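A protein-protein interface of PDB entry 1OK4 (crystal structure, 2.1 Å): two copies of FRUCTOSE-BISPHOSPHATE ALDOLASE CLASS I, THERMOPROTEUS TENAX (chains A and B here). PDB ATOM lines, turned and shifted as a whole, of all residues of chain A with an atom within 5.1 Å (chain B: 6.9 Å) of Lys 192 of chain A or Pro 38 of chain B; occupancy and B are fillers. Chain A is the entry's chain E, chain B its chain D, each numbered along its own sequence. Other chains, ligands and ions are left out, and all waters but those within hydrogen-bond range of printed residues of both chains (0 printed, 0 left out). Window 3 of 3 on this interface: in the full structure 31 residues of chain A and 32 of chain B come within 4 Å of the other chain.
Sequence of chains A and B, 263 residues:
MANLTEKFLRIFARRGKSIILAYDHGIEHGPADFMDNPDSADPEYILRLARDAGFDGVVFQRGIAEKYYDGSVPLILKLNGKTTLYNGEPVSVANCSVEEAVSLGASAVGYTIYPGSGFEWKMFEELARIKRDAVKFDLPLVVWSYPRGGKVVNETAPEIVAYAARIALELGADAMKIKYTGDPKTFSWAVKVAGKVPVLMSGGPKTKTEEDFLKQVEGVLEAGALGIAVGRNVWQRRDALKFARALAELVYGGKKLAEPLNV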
ATOM      1  N   SER A 188      13.915  22.424  -2.842  1.00  0.00           N
ATOM      2  CA  SER A 188      14.013  23.840  -3.190  1.00  0.00           C
ATOM      3  C   SER A 188      13.405  24.150  -4.571  1.00  0.00           C
ATOM      4  O   SER A 188      13.002  25.278  -4.815  1.00  0.00           O
ATOM      5  CB  SER A 188      15.460  24.325  -3.142  1.00  0.00           C
ATOM      6  OG  SER A 188      16.152  23.888  -4.286  1.00  0.00           O
ATOM      7  N   TRP A 189      13.349  23.168  -5.466  1.00  0.00           N
ATOM      8  CA  TRP A 189      12.605  23.312  -6.729  1.00  0.00           C
ATOM      9  C   TRP A 189      11.077  23.475  -6.467  1.00  0.00           C
ATOM     10  O   TRP A 189      10.433  24.353  -7.030  1.00  0.00           O
ATOM     11  CB  TRP A 189      12.886  22.114  -7.662  1.00  0.00           C
ATOM     12  CG  TRP A 189      12.146  22.156  -8.981  1.00  0.00           C
ATOM     13  CD1 TRP A 189      11.296  21.208  -9.473  1.00  0.00           C
ATOM     14  CD2 TRP A 189      12.189  23.202  -9.968  1.00  0.00           C
ATOM     15  NE1 TRP A 189      10.811  21.596 -10.699  1.00  0.00           N
ATOM     16  CE2 TRP A 189      11.337  22.815 -11.028  1.00  0.00           C
ATOM     17  CE3 TRP A 189      12.859  24.432 -10.064  1.00  0.00           C
ATOM     18  CZ2 TRP A 189      11.140  23.605 -12.173  1.00  0.00           C
ATOM     19  CZ3 TRP A 189      12.664  25.222 -11.201  1.00  0.00           C
ATOM     20  CH2 TRP A 189      11.812  24.801 -12.242  1.00  0.00           C
ATOM     21  N   ALA A 190      10.524  22.662  -5.578  1.00  0.00           N
ATOM     22  CA  ALA A 190       9.143  22.824  -5.164  1.00  0.00           C
ATOM     23  C   ALA A 190       8.873  24.210  -4.569  1.00  0.00           C
ATOM     24  O   ALA A 190       7.885  24.869  -4.902  1.00  0.00           O
ATOM     25  CB  ALA A 190       8.755  21.746  -4.193  1.00  0.00           C
ATOM     26  N   VAL A 191       9.759  24.663  -3.695  1.00  0.00           N
ATOM     27  CA  VAL A 191       9.640  25.977  -3.092  1.00  0.00           C
ATOM     28  C   VAL A 191       9.701  27.073  -4.149  1.00  0.00           C
ATOM     29  O   VAL A 191       8.938  28.038  -4.090  1.00  0.00           O
ATOM     30  CB  VAL A 191      10.755  26.214  -2.041  1.00  0.00           C
ATOM     31  CG1 VAL A 191      10.804  27.674  -1.613  1.00  0.00           C
ATOM     32  CG2 VAL A 191      10.536  25.308  -0.823  1.00  0.00           C
ATOM     33  N   LYS A 192      10.592  26.917  -5.122  1.00  0.00           N
ATOM     34  CA  LYS A 192      10.738  27.899  -6.182  1.00  0.00           C
ATOM     35  C   LYS A 192       9.479  28.003  -7.051  1.00  0.00           C
ATOM     36  O   LYS A 192       9.054  29.111  -7.357  1.00  0.00           O
ATOM     37  CB  LYS A 192      11.938  27.576  -7.061  1.00  0.00           C
ATOM     38  CG  LYS A 192      12.190  28.599  -8.182  1.00  0.00           C
ATOM     39  CD  LYS A 192      13.693  28.742  -8.479  1.00  0.00           C
ATOM     40  CE  LYS A 192      14.004  29.505  -9.810  1.00  0.00           C
ATOM     41  NZ  LYS A 192      12.823  30.227 -10.422  1.00  0.00           N
ATOM     42  N   VAL A 193       8.894  26.871  -7.451  1.00  0.00           N
ATOM     43  CA  VAL A 193       7.737  26.919  -8.349  1.00  0.00           C
ATOM     44  C   VAL A 193       6.487  27.401  -7.612  1.00  0.00           C
ATOM     45  O   VAL A 193       5.511  27.778  -8.245  1.00  0.00           O
ATOM     46  CB  VAL A 193       7.457  25.557  -9.078  1.00  0.00           C
ATOM     47  CG1 VAL A 193       8.649  25.151  -9.898  1.00  0.00           C
ATOM     48  CG2 VAL A 193       7.069  24.444  -8.105  1.00  0.00           C
ATOM     49  N   ALA A 194       6.522  27.368  -6.276  1.00  0.00           N
ATOM     50  CA  ALA A 194       5.448  27.931  -5.450  1.00  0.00           C
ATOM     51  C   ALA A 194       5.454  29.450  -5.451  1.00  0.00           C
ATOM     52  O   ALA A 194       4.479  30.074  -5.042  1.00  0.00           O
ATOM     53  CB  ALA A 194       5.548  27.419  -4.014  1.00  0.00           C
ATOM     54  N   GLY A 195       6.546  30.039  -5.911  1.00  0.00           N
ATOM     55  CA  GLY A 195       6.628  31.472  -6.092  1.00  0.00           C
ATOM     56  C   GLY A 195       6.405  32.230  -4.792  1.00  0.00           C
ATOM     57  O   GLY A 195       7.042  31.945  -3.795  1.00  0.00           O
ATOM     58  N   PHE B  34       9.045  23.696 -16.998  1.00  0.00           N
ATOM     59  CA  PHE B  34       9.888  24.869 -16.714  1.00  0.00           C
ATOM     60  C   PHE B  34      11.385  24.577 -16.579  1.00  0.00           C
ATOM     61  O   PHE B  34      12.162  25.497 -16.401  1.00  0.00           O
ATOM     62  CB  PHE B  34       9.431  25.594 -15.429  1.00  0.00           C
ATOM     63  CG  PHE B  34       7.961  25.951 -15.396  1.00  0.00           C
ATOM     64  CD1 PHE B  34       7.289  26.390 -16.539  1.00  0.00           C
ATOM     65  CD2 PHE B  34       7.256  25.858 -14.205  1.00  0.00           C
ATOM     66  CE1 PHE B  34       5.944  26.716 -16.495  1.00  0.00           C
ATOM     67  CE2 PHE B  34       5.921  26.182 -14.156  1.00  0.00           C
ATOM     68  CZ  PHE B  34       5.254  26.610 -15.319  1.00  0.00           C
ATOM     69  N   MET B  35      11.793  23.314 -16.660  1.00  0.00           N
ATOM     70  CA  MET B  35      13.205  22.947 -16.422  1.00  0.00           C
ATOM     71  C   MET B  35      14.160  23.391 -17.541  1.00  0.00           C
ATOM     72  O   MET B  35      15.277  23.815 -17.260  1.00  0.00           O
ATOM     73  CB  MET B  35      13.346  21.437 -16.184  1.00  0.00           C
ATOM     74  CG  MET B  35      12.696  20.960 -14.878  1.00  0.00           C
ATOM     75  SD  MET B  35      13.881  20.486 -13.589  1.00  0.00           S
ATOM     76  CE  MET B  35      14.868  22.064 -13.247  1.00  0.00           C
ATOM     77  N   ASP B  36      13.702  23.303 -18.792  1.00  0.00           N
ATOM     78  CA  ASP B  36      14.463  23.764 -19.963  1.00  0.00           C
ATOM     79  C   ASP B  36      14.957  25.222 -19.845  1.00  0.00           C
ATOM     80  O   ASP B  36      16.104  25.532 -20.215  1.00  0.00           O
ATOM     81  CB  ASP B  36      13.606  23.641 -21.241  1.00  0.00           C
ATOM     82  CG  ASP B  36      13.597  22.222 -21.836  1.00  0.00           C
ATOM     83  OD1 ASP B  36      14.245  21.314 -21.272  1.00  0.00           O
ATOM     84  OD2 ASP B  36      12.970  21.930 -22.880  1.00  0.00           O
ATOM     85  N   ASN B  37      14.077  26.100 -19.353  1.00  0.00           N
ATOM     86  CA  ASN B  37      14.361  27.522 -19.163  1.00  0.00           C
ATOM     87  C   ASN B  37      13.795  27.974 -17.802  1.00  0.00           C
ATOM     88  O   ASN B  37      12.674  28.477 -17.743  1.00  0.00           O
ATOM     89  CB  ASN B  37      13.753  28.317 -20.327  1.00  0.00           C
ATOM     90  CG  ASN B  37      13.959  29.819 -20.195  1.00  0.00           C
ATOM     91  OD1 ASN B  37      14.984  30.274 -19.690  1.00  0.00           O
ATOM     92  ND2 ASN B  37      12.984  30.595 -20.663  1.00  0.00           N
ATOM     93  N   PRO B  38      14.550  27.774 -16.714  1.00  0.00           N
ATOM     94  CA  PRO B  38      14.012  27.922 -15.347  1.00  0.00           C
ATOM     95  C   PRO B  38      13.330  29.247 -15.005  1.00  0.00           C
ATOM     96  O   PRO B  38      12.463  29.244 -14.128  1.00  0.00           O
ATOM     97  CB  PRO B  38      15.233  27.697 -14.453  1.00  0.00           C
ATOM     98  CG  PRO B  38      16.166  26.903 -15.292  1.00  0.00           C
ATOM     99  CD  PRO B  38      15.967  27.373 -16.698  1.00  0.00           C
ATOM    100  N   ASP B  39      13.689  30.337 -15.676  1.00  0.00           N
ATOM    101  CA  ASP B  39      13.001  31.612 -15.482  1.00  0.00           C
ATOM    102  C   ASP B  39      11.504  31.524 -15.767  1.00  0.00           C
ATOM    103  O   ASP B  39      10.733  32.309 -15.226  1.00  0.00           O
ATOM    104  CB  ASP B  39      13.586  32.698 -16.384  1.00  0.00           C
ATOM    105  CG  ASP B  39      15.001  33.107 -15.988  1.00  0.00           C
ATOM    106  OD1 ASP B  39      15.371  32.996 -14.793  1.00  0.00           O
ATOM    107  OD2 ASP B  39      15.808  33.561 -16.821  1.00  0.00           O
ATOM    108  N   SER B  40      11.126  30.592 -16.642  1.00  0.00           N
ATOM    109  CA  SER B  40       9.740  30.355 -17.032  1.00  0.00           C
ATOM    110  C   SER B  40       8.818  29.963 -15.883  1.00  0.00           C
ATOM    111  O   SER B  40       7.587  30.055 -16.008  1.00  0.00           O
ATOM    112  CB  SER B  40       9.680  29.282 -18.140  1.00  0.00           C
ATOM    113  OG  SER B  40      10.117  28.014 -17.668  1.00  0.00           O
ATOM    114  N   ALA B  41       9.392  29.507 -14.780  1.00  0.00           N
ATOM    115  CA  ALA B  41       8.623  29.215 -13.572  1.00  0.00           C
ATOM    116  C   ALA B  41       8.145  30.475 -12.846  1.00  0.00           C
ATOM    117  O   ALA B  41       7.249  30.401 -12.013  1.00  0.00           O
ATOM    118  CB  ALA B  41       9.450  28.374 -12.632  1.00  0.00           C
ATOM    119  N   ASP B  42       8.746  31.621 -13.167  1.00  0.00           N
ATOM    120  CA  ASP B  42       8.409  32.908 -12.569  1.00  0.00           C
ATOM    121  C   ASP B  42       7.375  33.673 -13.441  1.00  0.00           C
ATOM    122  O   ASP B  42       7.703  34.104 -14.539  1.00  0.00           O
ATOM    123  CB  ASP B  42       9.698  33.713 -12.438  1.00  0.00           C
ATOM    124  CG  ASP B  42       9.509  35.023 -11.729  1.00  0.00           C
ATOM    125  OD1 ASP B  42       8.353  35.337 -11.330  1.00  0.00           O
ATOM    126  OD2 ASP B  42      10.479  35.801 -11.537  1.00  0.00           O
ATOM    127  N   TYR B  45       8.556  37.003 -14.991  1.00  0.00           N
ATOM    128  CA  TYR B  45       9.304  36.807 -16.224  1.00  0.00           C
ATOM    129  C   TYR B  45       8.382  36.610 -17.438  1.00  0.00           C
ATOM    130  O   TYR B  45       8.662  37.109 -18.516  1.00  0.00           O
ATOM    131  CB  TYR B  45      10.264  35.629 -16.068  1.00  0.00           C
ATOM    132  CG  TYR B  45      10.851  35.110 -17.367  1.00  0.00           C
ATOM    133  CD1 TYR B  45      11.925  35.748 -17.969  1.00  0.00           C
ATOM    134  CD2 TYR B  45      10.337  33.974 -17.985  1.00  0.00           C
ATOM    135  CE1 TYR B  45      12.478  35.271 -19.157  1.00  0.00           C
ATOM    136  CE2 TYR B  45      10.883  33.491 -19.159  1.00  0.00           C
ATOM    137  CZ  TYR B  45      11.954  34.144 -19.745  1.00  0.00           C
ATOM    138  OH  TYR B  45      12.508  33.661 -20.914  1.00  0.00           O
ATOM    139  N   TYR B  68       0.119  37.694  -9.188  1.00  0.00           N
ATOM    140  CA  TYR B  68       1.100  38.304 -10.101  1.00  0.00           C
ATOM    141  C   TYR B  68       0.571  39.290 -11.119  1.00  0.00           C
ATOM    142  O   TYR B  68       1.342  40.114 -11.584  1.00  0.00           O
ATOM    143  CB  TYR B  68       1.852  37.213 -10.859  1.00  0.00           C
ATOM    144  CG  TYR B  68       2.722  36.356  -9.986  1.00  0.00           C
ATOM    145  CD1 TYR B  68       4.061  36.681  -9.773  1.00  0.00           C
ATOM    146  CD2 TYR B  68       2.209  35.216  -9.369  1.00  0.00           C
ATOM    147  CE1 TYR B  68       4.875  35.891  -8.942  1.00  0.00           C
ATOM    148  CE2 TYR B  68       2.997  34.420  -8.568  1.00  0.00           C
ATOM    149  CZ  TYR B  68       4.321  34.750  -8.357  1.00  0.00           C
ATOM    150  OH  TYR B  68       5.099  33.954  -7.550  1.00  0.00           O
ATOM    151  N   TRP B 235       8.396  30.222 -24.184  1.00  0.00           N
ATOM    152  CA  TRP B 235       9.084  30.281 -22.883  1.00  0.00           C
ATOM    153  C   TRP B 235       9.900  29.042 -22.478  1.00  0.00           C
ATOM    154  O   TRP B 235      10.600  29.073 -21.457  1.00  0.00           O
ATOM    155  CB  TRP B 235       8.146  30.721 -21.747  1.00  0.00           C
ATOM    156  CG  TRP B 235       6.865  29.996 -21.602  1.00  0.00           C
ATOM    157  CD1 TRP B 235       5.628  30.502 -21.827  1.00  0.00           C
ATOM    158  CD2 TRP B 235       6.668  28.657 -21.114  1.00  0.00           C
ATOM    159  NE1 TRP B 235       4.674  29.564 -21.532  1.00  0.00           N
ATOM    160  CE2 TRP B 235       5.285  28.418 -21.106  1.00  0.00           C
ATOM    161  CE3 TRP B 235       7.526  27.634 -20.689  1.00  0.00           C
ATOM    162  CZ2 TRP B 235       4.732  27.208 -20.700  1.00  0.00           C
ATOM    163  CZ3 TRP B 235       6.986  26.431 -20.286  1.00  0.00           C
ATOM    164  CH2 TRP B 235       5.589  26.218 -20.306  1.00  0.00           C
ATOM    165  N   ARG B 238      15.619  29.153 -24.314  1.00  0.00           N
ATOM    166  CA  ARG B 238      16.515  30.043 -23.580  1.00  0.00           C
ATOM    167  C   ARG B 238      16.677  31.400 -24.296  1.00  0.00           C
ATOM    168  O   ARG B 238      16.971  32.414 -23.656  1.00  0.00           O
ATOM    169  CB  ARG B 238      17.842  29.338 -23.323  1.00  0.00           C
ATOM    170  CG  ARG B 238      17.713  28.148 -22.342  1.00  0.00           C
ATOM    171  CD  ARG B 238      18.988  27.897 -21.521  1.00  0.00           C
ATOM    172  NE  ARG B 238      18.791  27.297 -20.188  1.00  0.00           N
ATOM    173  CZ  ARG B 238      19.264  26.105 -19.780  1.00  0.00           C
ATOM    174  NH1 ARG B 238      19.965  25.313 -20.597  1.00  0.00           N
ATOM    175  NH2 ARG B 238      19.022  25.695 -18.535  1.00  0.00           N
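Pro 38 of chain B touches Lys 192 of chain A. Gly 195 of chain A touches Tyr 68 of chain B.
Lys 192 of chain A touches one residue of chain B. Of chain A, only Lys 192 (3.9 Å) comes within 4 Å of Pro 38 of chain B. Printed residues of chain A within 4 Å of Tyr 68 of chain B: Gly 195 (3.3 Å). Of the printed residues of chain B, Gly 195 of chain A touches Tyr 68. Phe 34 of chain B touches none of the printed residues of chain A. Tyr 45 of chain B touches none of the printed residues of chain A. The nearest residue of chain B that does not touch Lys 192 of chain A is Ala 41 of chain B (4.4 Å).
Along chain A the printed residues that touch a printed residue of chain B span positions 192 to 195. Of the 13 printed residues of chain B, 2 touch a printed residue of chain A. Hydrophobic or aromatic side chains of chain B within 4 Å of the printed part of chain A: Tyr 68. Along chain B the printed residues that touch a printed residue of chain A span positions 38 to 68. Among the printed residues, no Asp or Glu carboxylate lies within 4 Å of a Lys or Arg side-chain nitrogen of the other chain.
No position is printed for both chains. Of the 2 pairs that touch across the chains among the printed residues, none has its exchanged pair printed and touching as well.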
